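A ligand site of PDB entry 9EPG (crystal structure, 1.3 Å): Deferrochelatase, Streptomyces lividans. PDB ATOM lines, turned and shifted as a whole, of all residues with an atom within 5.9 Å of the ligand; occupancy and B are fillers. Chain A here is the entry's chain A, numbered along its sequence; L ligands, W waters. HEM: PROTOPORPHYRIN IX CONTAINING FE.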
ATOM      1  N   ASN A 186     -24.805   5.968  21.304  1.00  0.00           N
ATOM      2  CA  ASN A 186     -24.646   5.949  19.854  1.00  0.00           C
ATOM      3  C   ASN A 186     -23.545   4.945  19.503  1.00  0.00           C
ATOM      4  O   ASN A 186     -22.958   4.328  20.375  1.00  0.00           O
ATOM      5  CB  ASN A 186     -24.400   7.337  19.298  1.00  0.00           C
ATOM      6  CG  ASN A 186     -23.179   7.972  19.897  1.00  0.00           C
ATOM      7  OD1 ASN A 186     -22.132   7.341  20.065  1.00  0.00           O
ATOM      8  ND2 ASN A 186     -23.312   9.224  20.303  1.00  0.00           N
ATOM      9  N   LEU A 188     -20.626   5.393  18.419  1.00  0.00           N
ATOM     10  CA  LEU A 188     -19.291   5.737  18.887  1.00  0.00           C
ATOM     11  C   LEU A 188     -19.085   5.315  20.331  1.00  0.00           C
ATOM     12  O   LEU A 188     -17.992   5.479  20.880  1.00  0.00           O
ATOM     13  CB  LEU A 188     -19.027   7.210  18.700  1.00  0.00           C
ATOM     14  CG  LEU A 188     -19.176   7.764  17.302  1.00  0.00           C
ATOM     15  CD1 LEU A 188     -18.780   9.238  17.238  1.00  0.00           C
ATOM     16  CD2 LEU A 188     -18.406   6.958  16.287  1.00  0.00           C
ATOM     17  N   PHE A 190     -20.705   6.502  23.086  1.00  0.00           N
ATOM     18  CA  PHE A 190     -21.007   7.523  24.087  1.00  0.00           C
ATOM     19  C   PHE A 190     -22.497   7.640  24.287  1.00  0.00           C
ATOM     20  O   PHE A 190     -23.270   7.546  23.343  1.00  0.00           O
ATOM     21  CB  PHE A 190     -20.472   8.875  23.616  1.00  0.00           C
ATOM     22  CG  PHE A 190     -19.001   9.028  23.917  1.00  0.00           C
ATOM     23  CD1 PHE A 190     -18.024   8.421  23.145  1.00  0.00           C
ATOM     24  CD2 PHE A 190     -18.533   9.815  24.979  1.00  0.00           C
ATOM     25  CE1 PHE A 190     -16.680   8.550  23.423  1.00  0.00           C
ATOM     26  CE2 PHE A 190     -17.178   9.917  25.251  1.00  0.00           C
ATOM     27  CZ  PHE A 190     -16.259   9.303  24.486  1.00  0.00           C
ATOM     28  N   LYS A 191     -22.898   7.934  25.527  1.00  0.00           N
ATOM     29  CA  LYS A 191     -24.259   8.293  25.837  1.00  0.00           C
ATOM     30  C   LYS A 191     -24.628   9.534  25.043  1.00  0.00           C
ATOM     31  O   LYS A 191     -23.836  10.468  24.945  1.00  0.00           O
ATOM     32  CB  LYS A 191     -24.393   8.606  27.338  1.00  0.00           C
ATOM     33  CG  LYS A 191     -24.219   7.438  28.242  1.00  0.00           C
ATOM     34  CD  LYS A 191     -24.256   7.843  29.730  1.00  0.00           C
ATOM     35  CE  LYS A 191     -24.155   6.668  30.677  1.00  0.00           C
ATOM     36  NZ  LYS A 191     -24.171   7.098  32.098  1.00  0.00           N
ATOM     37  N   ASP A 192     -25.837   9.562  24.506  1.00  0.00           N
ATOM     38  CA  ASP A 192     -26.296  10.636  23.641  1.00  0.00           C
ATOM     39  C   ASP A 192     -27.716  10.934  24.057  1.00  0.00           C
ATOM     40  O   ASP A 192     -28.611  10.102  23.911  1.00  0.00           O
ATOM     41  CB  ASP A 192     -26.150  10.170  22.191  1.00  0.00           C
ATOM     42  CG  ASP A 192     -26.103  11.278  21.157  1.00  0.00           C
ATOM     43  OD1 ASP A 192     -26.447  12.434  21.437  1.00  0.00           O
ATOM     44  OD2 ASP A 192     -25.658  10.924  20.046  1.00  0.00           O
ATOM     45  N   GLY A 193     -27.903  12.126  24.613  1.00  0.00           N
ATOM     46  CA  GLY A 193     -29.200  12.546  25.082  1.00  0.00           C
ATOM     47  C   GLY A 193     -29.234  13.075  26.504  1.00  0.00           C
ATOM     48  O   GLY A 193     -30.296  13.474  26.946  1.00  0.00           O
ATOM     49  N   THR A 194     -28.095  13.162  27.206  1.00  0.00           N
ATOM     50  CA  THR A 194     -28.111  13.601  28.583  1.00  0.00           C
ATOM     51  C   THR A 194     -28.731  14.976  28.737  1.00  0.00           C
ATOM     52  O   THR A 194     -29.589  15.176  29.601  1.00  0.00           O
ATOM     53  CB  THR A 194     -26.678  13.562  29.078  1.00  0.00           C
ATOM     54  OG1 THR A 194     -26.125  12.266  28.926  1.00  0.00           O
ATOM     55  CG2 THR A 194     -26.599  14.035  30.507  1.00  0.00           C
ATOM     56  N   ARG A 195     -28.232  15.971  27.992  1.00  0.00           N
ATOM     57  CA  ARG A 195     -28.701  17.337  28.104  1.00  0.00           C
ATOM     58  C   ARG A 195     -29.580  17.676  26.910  1.00  0.00           C
ATOM     59  O   ARG A 195     -29.139  18.271  25.938  1.00  0.00           O
ATOM     60  CB  ARG A 195     -27.548  18.317  28.286  1.00  0.00           C
ATOM     61  CG  ARG A 195     -27.073  18.398  29.733  1.00  0.00           C
ATOM     62  CD  ARG A 195     -25.949  19.330  30.000  1.00  0.00           C
ATOM     63  NE  ARG A 195     -26.072  20.591  29.294  1.00  0.00           N
ATOM     64  CZ  ARG A 195     -27.012  21.487  29.509  1.00  0.00           C
ATOM     65  NH1 ARG A 195     -27.225  22.344  28.560  1.00  0.00           N
ATOM     66  NH2 ARG A 195     -27.694  21.558  30.639  1.00  0.00           N
ATOM     67  N   ASN A 196     -30.815  17.208  26.970  1.00  0.00           N
ATOM     68  CA  ASN A 196     -31.803  17.439  25.959  1.00  0.00           C
ATOM     69  C   ASN A 196     -32.911  18.314  26.571  1.00  0.00           C
ATOM     70  O   ASN A 196     -32.611  19.249  27.315  1.00  0.00           O
ATOM     71  CB  ASN A 196     -32.180  16.099  25.328  1.00  0.00           C
ATOM     72  CG  ASN A 196     -32.869  16.245  24.013  1.00  0.00           C
ATOM     73  OD1 ASN A 196     -32.537  17.138  23.229  1.00  0.00           O
ATOM     74  ND2 ASN A 196     -33.822  15.401  23.733  1.00  0.00           N
ATOM     75  N   ARG A 229     -30.811  15.112   9.469  1.00  0.00           N
ATOM     76  CA  ARG A 229     -29.508  15.019   8.834  1.00  0.00           C
ATOM     77  C   ARG A 229     -29.037  13.591   8.910  1.00  0.00           C
ATOM     78  O   ARG A 229     -28.983  12.990   9.993  1.00  0.00           O
ATOM     79  CB  ARG A 229     -28.467  15.891   9.537  1.00  0.00           C
ATOM     80  CG  ARG A 229     -28.778  17.368   9.553  1.00  0.00           C
ATOM     81  CD  ARG A 229     -28.698  18.081   8.211  1.00  0.00           C
ATOM     82  NE  ARG A 229     -27.267  18.284   7.925  1.00  0.00           N
ATOM     83  CZ  ARG A 229     -26.793  19.146   7.062  1.00  0.00           C
ATOM     84  NH1 ARG A 229     -27.592  19.819   6.260  1.00  0.00           N
ATOM     85  NH2 ARG A 229     -25.482  19.298   6.975  1.00  0.00           N
ATOM     86  N   ILE A 231     -26.070  11.210   8.894  1.00  0.00           N
ATOM     87  CA  ILE A 231     -24.663  11.404   9.199  1.00  0.00           C
ATOM     88  C   ILE A 231     -23.964  10.063   9.189  1.00  0.00           C
ATOM     89  O   ILE A 231     -24.254   9.200  10.002  1.00  0.00           O
ATOM     90  CB  ILE A 231     -24.496  12.098  10.555  1.00  0.00           C
ATOM     91  CG1 ILE A 231     -25.294  13.384  10.576  1.00  0.00           C
ATOM     92  CG2 ILE A 231     -23.011  12.406  10.838  1.00  0.00           C
ATOM     93  CD1 ILE A 231     -25.284  14.149  11.905  1.00  0.00           C
ATOM     94  N   MET A 233     -20.751   7.805   9.969  1.00  0.00           N
ATOM     95  CA  MET A 233     -19.659   7.781  10.936  1.00  0.00           C
ATOM     96  C   MET A 233     -18.487   7.016  10.352  1.00  0.00           C
ATOM     97  O   MET A 233     -18.656   5.938   9.821  1.00  0.00           O
ATOM     98  CB  MET A 233     -20.103   7.066  12.227  1.00  0.00           C
ATOM     99  CG  MET A 233     -21.077   7.883  13.019  1.00  0.00           C
ATOM    100  SD  MET A 233     -21.837   6.828  14.293  1.00  0.00           S
ATOM    101  CE  MET A 233     -22.418   8.054  15.463  1.00  0.00           C
ATOM    102  N   PHE A 250     -15.422  14.798  22.779  1.00  0.00           N
ATOM    103  CA  PHE A 250     -16.726  15.128  23.312  1.00  0.00           C
ATOM    104  C   PHE A 250     -16.714  16.104  24.496  1.00  0.00           C
ATOM    105  O   PHE A 250     -17.591  16.958  24.598  1.00  0.00           O
ATOM    106  CB  PHE A 250     -17.515  13.873  23.701  1.00  0.00           C
ATOM    107  CG  PHE A 250     -18.024  13.190  22.455  1.00  0.00           C
ATOM    108  CD1 PHE A 250     -19.003  13.814  21.716  1.00  0.00           C
ATOM    109  CD2 PHE A 250     -17.552  11.963  22.047  1.00  0.00           C
ATOM    110  CE1 PHE A 250     -19.456  13.259  20.538  1.00  0.00           C
ATOM    111  CE2 PHE A 250     -18.045  11.391  20.884  1.00  0.00           C
ATOM    112  CZ  PHE A 250     -18.974  12.059  20.144  1.00  0.00           C
ATOM    113  N   ARG A 252     -16.783  14.689  27.571  1.00  0.00           N
ATOM    114  CA  ARG A 252     -17.358  13.825  28.575  1.00  0.00           C
ATOM    115  C   ARG A 252     -16.564  12.539  28.563  1.00  0.00           C
ATOM    116  O   ARG A 252     -16.005  12.191  27.536  1.00  0.00           O
ATOM    117  CB  ARG A 252     -18.827  13.503  28.321  1.00  0.00           C
ATOM    118  CG  ARG A 252     -19.730  14.693  28.560  1.00  0.00           C
ATOM    119  CD  ARG A 252     -21.160  14.415  28.224  1.00  0.00           C
ATOM    120  NE  ARG A 252     -22.082  15.499  28.532  1.00  0.00           N
ATOM    121  CZ  ARG A 252     -22.732  15.675  29.675  1.00  0.00           C
ATOM    122  NH1 ARG A 252     -22.546  14.874  30.699  1.00  0.00           N
ATOM    123  NH2 ARG A 252     -23.625  16.646  29.746  1.00  0.00           N
ATOM    124  N   PRO A 269     -21.995  20.473  32.978  1.00  0.00           N
ATOM    125  CA  PRO A 269     -20.703  20.715  32.389  1.00  0.00           C
ATOM    126  C   PRO A 269     -20.058  21.998  32.877  1.00  0.00           C
ATOM    127  O   PRO A 269     -20.767  22.986  33.029  1.00  0.00           O
ATOM    128  CB  PRO A 269     -20.948  20.825  30.900  1.00  0.00           C
ATOM    129  CG  PRO A 269     -22.399  20.650  30.717  1.00  0.00           C
ATOM    130  CD  PRO A 269     -23.115  20.368  32.044  1.00  0.00           C
ATOM    131  N   HIS A 279     -17.041  18.770  21.250  1.00  0.00           N
ATOM    132  CA  HIS A 279     -18.412  18.825  20.749  1.00  0.00           C
ATOM    133  C   HIS A 279     -19.363  19.463  21.752  1.00  0.00           C
ATOM    134  O   HIS A 279     -20.180  20.284  21.377  1.00  0.00           O
ATOM    135  CB  HIS A 279     -18.819  17.419  20.347  1.00  0.00           C
ATOM    136  CG  HIS A 279     -20.196  17.322  19.824  1.00  0.00           C
ATOM    137  ND1 HIS A 279     -20.557  17.744  18.585  1.00  0.00           N
ATOM    138  CD2 HIS A 279     -21.329  16.806  20.367  1.00  0.00           C
ATOM    139  CE1 HIS A 279     -21.860  17.493  18.415  1.00  0.00           C
ATOM    140  NE2 HIS A 279     -22.365  16.936  19.468  1.00  0.00           N
ATOM    141  N   VAL A 280     -19.333  19.006  23.019  1.00  0.00           N
ATOM    142  CA  VAL A 280     -20.271  19.540  23.996  1.00  0.00           C
ATOM    143  C   VAL A 280     -20.049  21.033  24.205  1.00  0.00           C
ATOM    144  O   VAL A 280     -21.027  21.769  24.351  1.00  0.00           O
ATOM    145  CB  VAL A 280     -20.186  18.742  25.303  1.00  0.00           C
ATOM    146  CG1 VAL A 280     -20.926  19.431  26.431  1.00  0.00           C
ATOM    147  CG2 VAL A 280     -20.683  17.316  25.102  1.00  0.00           C
ATOM    148  N   ALA A 283     -21.540  22.848  21.219  1.00  0.00           N
ATOM    149  CA  ALA A 283     -22.967  22.681  20.992  1.00  0.00           C
ATOM    150  C   ALA A 283     -23.811  23.204  22.131  1.00  0.00           C
ATOM    151  O   ALA A 283     -25.012  23.330  21.978  1.00  0.00           O
ATOM    152  CB  ALA A 283     -23.250  21.195  20.788  1.00  0.00           C
ATOM    153  N   HIS A 284     -23.224  23.477  23.307  1.00  0.00           N
ATOM    154  CA  HIS A 284     -23.983  23.823  24.497  1.00  0.00           C
ATOM    155  C   HIS A 284     -24.716  25.129  24.263  1.00  0.00           C
ATOM    156  O   HIS A 284     -24.176  26.008  23.604  1.00  0.00           O
ATOM    157  CB  HIS A 284     -22.991  24.004  25.647  1.00  0.00           C
ATOM    158  CG  HIS A 284     -23.573  24.084  26.985  1.00  0.00           C
ATOM    159  ND1 HIS A 284     -24.167  25.217  27.482  1.00  0.00           N
ATOM    160  CD2 HIS A 284     -23.661  23.152  27.977  1.00  0.00           C
ATOM    161  CE1 HIS A 284     -24.584  24.966  28.712  1.00  0.00           C
ATOM    162  NE2 HIS A 284     -24.262  23.726  29.059  1.00  0.00           N
ATOM    163  N   PRO A 285     -25.927  25.296  24.817  1.00  0.00           N
ATOM    164  CA  PRO A 285     -26.660  26.562  24.670  1.00  0.00           C
ATOM    165  C   PRO A 285     -25.854  27.795  25.066  1.00  0.00           C
ATOM    166  O   PRO A 285     -25.976  28.814  24.374  1.00  0.00           O
ATOM    167  CB  PRO A 285     -27.841  26.343  25.593  1.00  0.00           C
ATOM    168  CG  PRO A 285     -28.123  24.866  25.455  1.00  0.00           C
ATOM    169  CD  PRO A 285     -26.736  24.287  25.489  1.00  0.00           C
ATOM    170  N   LEU A 293     -32.068  22.774  21.444  1.00  0.00           N
ATOM    171  CA  LEU A 293     -32.766  21.905  20.511  1.00  0.00           C
ATOM    172  C   LEU A 293     -33.363  20.742  21.258  1.00  0.00           C
ATOM    173  O   LEU A 293     -32.858  20.369  22.298  1.00  0.00           O
ATOM    174  CB  LEU A 293     -31.725  21.278  19.571  1.00  0.00           C
ATOM    175  CG  LEU A 293     -30.849  22.222  18.776  1.00  0.00           C
ATOM    176  CD1 LEU A 293     -29.833  21.421  17.969  1.00  0.00           C
ATOM    177  CD2 LEU A 293     -31.715  23.062  17.876  1.00  0.00           C
ATOM    178  N   ARG A 295     -33.335  17.009  20.534  1.00  0.00           N
ATOM    179  CA  ARG A 295     -32.730  16.011  19.690  1.00  0.00           C
ATOM    180  C   ARG A 295     -33.476  14.705  19.836  1.00  0.00           C
ATOM    181  O   ARG A 295     -33.824  14.326  20.967  1.00  0.00           O
ATOM    182  CB  ARG A 295     -31.273  15.806  20.110  1.00  0.00           C
ATOM    183  CG  ARG A 295     -30.416  17.023  19.796  1.00  0.00           C
ATOM    184  CD  ARG A 295     -29.053  16.826  20.295  1.00  0.00           C
ATOM    185  NE  ARG A 295     -29.021  16.955  21.741  1.00  0.00           N
ATOM    186  CZ  ARG A 295     -28.310  16.218  22.570  1.00  0.00           C
ATOM    187  NH1 ARG A 295     -27.532  15.237  22.163  1.00  0.00           N
ATOM    188  NH2 ARG A 295     -28.362  16.452  23.868  1.00  0.00           N
ATOM    189  N   LEU A 314     -25.703   7.871  12.058  1.00  0.00           N
ATOM    190  CA  LEU A 314     -26.676   8.438  12.964  1.00  0.00           C
ATOM    191  C   LEU A 314     -27.625   9.272  12.126  1.00  0.00           C
ATOM    192  O   LEU A 314     -27.201  10.117  11.350  1.00  0.00           O
ATOM    193  CB  LEU A 314     -25.944   9.226  14.044  1.00  0.00           C
ATOM    194  CG  LEU A 314     -26.775   9.591  15.257  1.00  0.00           C
ATOM    195  CD1 LEU A 314     -25.964   9.710  16.480  1.00  0.00           C
ATOM    196  CD2 LEU A 314     -27.517  10.862  15.052  1.00  0.00           C
ATOM    197  N   PHE A 316     -29.865  12.011  12.515  1.00  0.00           N
ATOM    198  CA  PHE A 316     -30.035  13.077  13.475  1.00  0.00           C
ATOM    199  C   PHE A 316     -31.324  13.809  13.177  1.00  0.00           C
ATOM    200  O   PHE A 316     -31.572  14.205  12.065  1.00  0.00           O
ATOM    201  CB  PHE A 316     -28.850  14.038  13.288  1.00  0.00           C
ATOM    202  CG  PHE A 316     -28.874  15.198  14.268  1.00  0.00           C
ATOM    203  CD1 PHE A 316     -28.325  15.021  15.521  1.00  0.00           C
ATOM    204  CD2 PHE A 316     -29.455  16.401  13.950  1.00  0.00           C
ATOM    205  CE1 PHE A 316     -28.340  16.087  16.441  1.00  0.00           C
ATOM    206  CE2 PHE A 316     -29.487  17.427  14.884  1.00  0.00           C
ATOM    207  CZ  PHE A 316     -28.906  17.240  16.108  1.00  0.00           C
ATOM    208  N   PHE A 327     -31.255  24.859  14.981  1.00  0.00           N
ATOM    209  CA  PHE A 327     -30.210  24.075  14.351  1.00  0.00           C
ATOM    210  C   PHE A 327     -29.148  24.929  13.662  1.00  0.00           C
ATOM    211  O   PHE A 327     -27.973  24.602  13.750  1.00  0.00           O
ATOM    212  CB  PHE A 327     -30.849  23.137  13.335  1.00  0.00           C
ATOM    213  CG  PHE A 327     -29.884  22.289  12.550  1.00  0.00           C
ATOM    214  CD1 PHE A 327     -29.342  21.127  13.092  1.00  0.00           C
ATOM    215  CD2 PHE A 327     -29.413  22.694  11.320  1.00  0.00           C
ATOM    216  CE1 PHE A 327     -28.440  20.357  12.409  1.00  0.00           C
ATOM    217  CE2 PHE A 327     -28.495  21.906  10.634  1.00  0.00           C
ATOM    218  CZ  PHE A 327     -27.985  20.781  11.183  1.00  0.00           C
ATOM    219  N   VAL A 330     -26.345  26.406  15.959  1.00  0.00           N
ATOM    220  CA  VAL A 330     -25.566  25.389  16.604  1.00  0.00           C
ATOM    221  C   VAL A 330     -24.700  24.665  15.565  1.00  0.00           C
ATOM    222  O   VAL A 330     -23.507  24.508  15.780  1.00  0.00           O
ATOM    223  CB  VAL A 330     -26.496  24.443  17.375  1.00  0.00           C
ATOM    224  CG1 VAL A 330     -25.691  23.309  17.978  1.00  0.00           C
ATOM    225  CG2 VAL A 330     -27.272  25.169  18.464  1.00  0.00           C
ATOM    226  N   GLN A 331     -25.257  24.292  14.414  1.00  0.00           N
ATOM    227  CA  GLN A 331     -24.429  23.649  13.401  1.00  0.00           C
ATOM    228  C   GLN A 331     -23.324  24.577  12.906  1.00  0.00           C
ATOM    229  O   GLN A 331     -22.227  24.114  12.633  1.00  0.00           O
ATOM    230  CB  GLN A 331     -25.289  23.115  12.271  1.00  0.00           C
ATOM    231  CG  GLN A 331     -24.574  22.391  11.155  1.00  0.00           C
ATOM    232  CD  GLN A 331     -23.806  21.160  11.546  1.00  0.00           C
ATOM    233  OE1 GLN A 331     -24.211  20.416  12.438  1.00  0.00           O
ATOM    234  NE2 GLN A 331     -22.705  20.898  10.890  1.00  0.00           N
ATOM    235  N   LEU A 334     -20.447  24.325  14.997  1.00  0.00           N
ATOM    236  CA  LEU A 334     -19.747  23.051  14.932  1.00  0.00           C
ATOM    237  C   LEU A 334     -18.746  23.020  13.780  1.00  0.00           C
ATOM    238  O   LEU A 334     -18.145  21.982  13.525  1.00  0.00           O
ATOM    239  CB  LEU A 334     -20.702  21.863  14.842  1.00  0.00           C
ATOM    240  CG  LEU A 334     -21.643  21.731  16.034  1.00  0.00           C
ATOM    241  CD1 LEU A 334     -22.535  20.487  15.896  1.00  0.00           C
ATOM    242  CD2 LEU A 334     -20.961  21.635  17.345  1.00  0.00           C
ATOM    243  N   LEU A 339     -15.270  16.509  16.410  1.00  0.00           N
ATOM    244  CA  LEU A 339     -16.056  15.392  15.901  1.00  0.00           C
ATOM    245  C   LEU A 339     -16.089  15.347  14.377  1.00  0.00           C
ATOM    246  O   LEU A 339     -16.250  14.278  13.784  1.00  0.00           O
ATOM    247  CB  LEU A 339     -17.470  15.462  16.476  1.00  0.00           C
ATOM    248  CG  LEU A 339     -18.412  14.318  16.084  1.00  0.00           C
ATOM    249  CD1 LEU A 339     -17.896  12.982  16.594  1.00  0.00           C
ATOM    250  CD2 LEU A 339     -19.794  14.642  16.614  1.00  0.00           C
ATOM    251  N   ILE A 343     -17.075  12.173  11.061  1.00  0.00           N
ATOM    252  CA  ILE A 343     -18.446  12.124  10.562  1.00  0.00           C
ATOM    253  C   ILE A 343     -18.516  12.864   9.229  1.00  0.00           C
ATOM    254  O   ILE A 343     -17.640  13.647   8.885  1.00  0.00           O
ATOM    255  CB  ILE A 343     -19.450  12.746  11.551  1.00  0.00           C
ATOM    256  CG1 ILE A 343     -19.216  14.247  11.744  1.00  0.00           C
ATOM    257  CG2 ILE A 343     -19.426  11.976  12.864  1.00  0.00           C
ATOM    258  CD1 ILE A 343     -20.378  14.967  12.411  1.00  0.00           C
ATOM    259  N   HIS A 345     -21.924  14.609   6.946  1.00  0.00           N
ATOM    260  CA  HIS A 345     -23.346  14.724   6.663  1.00  0.00           C
ATOM    261  C   HIS A 345     -23.580  14.403   5.196  1.00  0.00           C
ATOM    262  O   HIS A 345     -22.966  15.038   4.332  1.00  0.00           O
ATOM    263  CB  HIS A 345     -23.793  16.129   6.970  1.00  0.00           C
ATOM    264  CG  HIS A 345     -23.733  16.521   8.392  1.00  0.00           C
ATOM    265  ND1 HIS A 345     -24.851  17.061   9.004  1.00  0.00           N
ATOM    266  CD2 HIS A 345     -22.771  16.524   9.323  1.00  0.00           C
ATOM    267  CE1 HIS A 345     -24.525  17.356  10.261  1.00  0.00           C
ATOM    268  NE2 HIS A 345     -23.251  17.071  10.459  1.00  0.00           N
HETATM  269  CHA HEM L   1     -24.429  16.507  22.923  1.00  0.00           C
HETATM  270  CHB HEM L   1     -22.765  12.993  20.078  1.00  0.00           C
HETATM  271  CHC HEM L   1     -24.276  15.426  16.177  1.00  0.00           C
HETATM  272  CHD HEM L   1     -25.971  18.875  19.086  1.00  0.00           C
HETATM  273  C1A HEM L   1     -23.807  15.343  22.515  1.00  0.00           C
HETATM  274  C2A HEM L   1     -23.243  14.378  23.370  1.00  0.00           C
HETATM  275  C3A HEM L   1     -22.744  13.373  22.588  1.00  0.00           C
HETATM  276  C4A HEM L   1     -23.042  13.731  21.236  1.00  0.00           C
HETATM  277  CMA HEM L   1     -22.017  12.130  22.972  1.00  0.00           C
HETATM  278  CAA HEM L   1     -23.115  14.446  24.882  1.00  0.00           C
HETATM  279  CBA HEM L   1     -24.333  13.933  25.671  1.00  0.00           C
HETATM  280  CGA HEM L   1     -25.559  14.757  25.487  1.00  0.00           C
HETATM  281  O1A HEM L   1     -26.404  14.411  24.624  1.00  0.00           O
HETATM  282  O2A HEM L   1     -25.788  15.753  26.214  1.00  0.00           O
HETATM  283  C1B HEM L   1     -23.055  13.372  18.762  1.00  0.00           C
HETATM  284  C2B HEM L   1     -22.735  12.539  17.635  1.00  0.00           C
HETATM  285  C3B HEM L   1     -23.158  13.209  16.551  1.00  0.00           C
HETATM  286  C4B HEM L   1     -23.723  14.475  16.994  1.00  0.00           C
HETATM  287  CMB HEM L   1     -22.061  11.199  17.679  1.00  0.00           C
HETATM  288  CAB HEM L   1     -23.151  12.877  15.114  1.00  0.00           C
HETATM  289  CBB HEM L   1     -22.930  11.716  14.660  1.00  0.00           C
HETATM  290  C1C HEM L   1     -24.857  16.598  16.614  1.00  0.00           C
HETATM  291  C2C HEM L   1     -25.366  17.620  15.793  1.00  0.00           C
HETATM  292  C3C HEM L   1     -25.858  18.602  16.612  1.00  0.00           C
HETATM  293  C4C HEM L   1     -25.581  18.191  17.944  1.00  0.00           C
HETATM  294  CMC HEM L   1     -25.462  17.556  14.296  1.00  0.00           C
HETATM  295  CAC HEM L   1     -26.510  19.874  16.294  1.00  0.00           C
HETATM  296  CBC HEM L   1     -26.382  20.541  15.225  1.00  0.00           C
HETATM  297  C1D HEM L   1     -25.756  18.444  20.391  1.00  0.00           C
HETATM  298  C2D HEM L   1     -26.221  19.205  21.553  1.00  0.00           C
HETATM  299  C3D HEM L   1     -25.776  18.579  22.646  1.00  0.00           C
HETATM  300  C4D HEM L   1     -25.019  17.429  22.122  1.00  0.00           C
HETATM  301  CMD HEM L   1     -27.053  20.452  21.516  1.00  0.00           C
HETATM  302  CAD HEM L   1     -25.993  18.976  24.054  1.00  0.00           C
HETATM  303  CBD HEM L   1     -24.940  20.013  24.584  1.00  0.00           C
HETATM  304  CGD HEM L   1     -25.222  20.447  25.963  1.00  0.00           C
HETATM  305  O1D HEM L   1     -24.598  19.941  26.926  1.00  0.00           O
HETATM  306  O2D HEM L   1     -26.174  21.237  26.120  1.00  0.00           O
HETATM  307  NA  HEM L   1     -23.697  14.905  21.180  1.00  0.00           N
HETATM  308  NB  HEM L   1     -23.642  14.486  18.343  1.00  0.00           N
HETATM  309  NC  HEM L   1     -24.973  16.978  17.914  1.00  0.00           N
HETATM  310  ND  HEM L   1     -25.053  17.371  20.773  1.00  0.00           N
HETATM  311 FE   HEM L   1     -24.247  16.004  19.585  1.00  0.00          FE
HETATM  312  O   HOH W   1     -23.773  17.379  27.033  1.00  0.00           O
HETATM  313  O   HOH W   2     -27.828  23.697  21.882  1.00  0.00           O
HETATM  314  O   HOH W   3     -28.832  21.040  25.522  1.00  0.00           O
HETATM  315  O   HOH W   4     -29.691  21.987  22.982  1.00  0.00           O
HETATM  316  O   HOH W   5     -26.117  14.660  19.747  1.00  0.00           O
HETATM  317  O   HOH W   6     -26.369  12.538  18.045  1.00  0.00           O
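The side-chain amide oxygen of Asn 196 is in hydrogen-bond range of the backbone NH of Arg 295 (2.8 Å). ND2 of Asn 186 sits at hydrogen-bond distance from OD2 of Asp 192 (2.9 Å). The backbone NH of Phe 316 lies within hydrogen-bond range of the backbone carbonyl oxygen of Arg 229, 2.8 Å away. N of Phe 190 sits at hydrogen-bond distance from OD1 of Asn 186 (3.4 Å). The side-chain carboxylate of Asp 192 is in salt-bridge range of the guanidinium group of Arg 295 (3.1 Å). The backbone carbonyl oxygen (O) of Phe 250 lies within hydrogen-bond range of the backbone NH (N) of Val 280, at 3.1 Å. N of Leu 314 is in hydrogen-bond range of O of Ile 231 (2.8 Å). The backbone NH (N) of Leu 188 is in hydrogen-bond range of the side-chain amide oxygen (OD1) of Asn 186 (3.0 Å).
Water W5 lies within hydrogen-bond range of OD1 of Asp 192 (2.8 Å) and NH1 of Arg 295 (2.9 Å). Water W1 bridges an oxygen (O1D) of the ligand (2.7 Å) and the guanidinium group of Arg 252 (2.8 Å). Water W3 lies within hydrogen-bond range of O2D of the ligand and O of Arg 195.
The guanidinium group (NH1) of Arg 295 is in salt-bridge range of an oxygen (O1A) of the ligand (2.8 Å). The backbone NH (N) of Gly 193 is in hydrogen-bond range of an oxygen (O1A) of the ligand, 2.7 Å away. The backbone NH of Thr 194 is in hydrogen-bond range of an oxygen (O1A) of the ligand. The backbone NH (N) of Arg 195 lies within hydrogen-bond range of an oxygen (O2A) of the ligand, 3.0 Å away. NE2 of His 279 binds FE of the ligand (2.1 Å). NE of Arg 195 is in salt-bridge range of O1D of the ligand (2.9 Å).
Residues that only touch the ligand: Asn 186, Leu 188, Phe 190, Lys 191, Asp 192, Ile 231, Met 233, Phe 250, Arg 252, Val 280, Ala 283, His 284, Pro 285, Leu 314, Phe 316, Phe 327, Val 330, Gln 331, Leu 334, Leu 339 and Ile 343. Hydrophobic or aromatic side chains that line the ligand: Leu 188, Phe 190, Ile 231, Met 233, Phe 250, His 279, Val 280, Ala 283, His 284, Pro 285, Leu 314, Phe 316, Phe 327, Val 330, Leu 334, Leu 339 and Ile 343. The nearest printed residue that does not touch the ligand is Leu 293 (4.03 Å).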
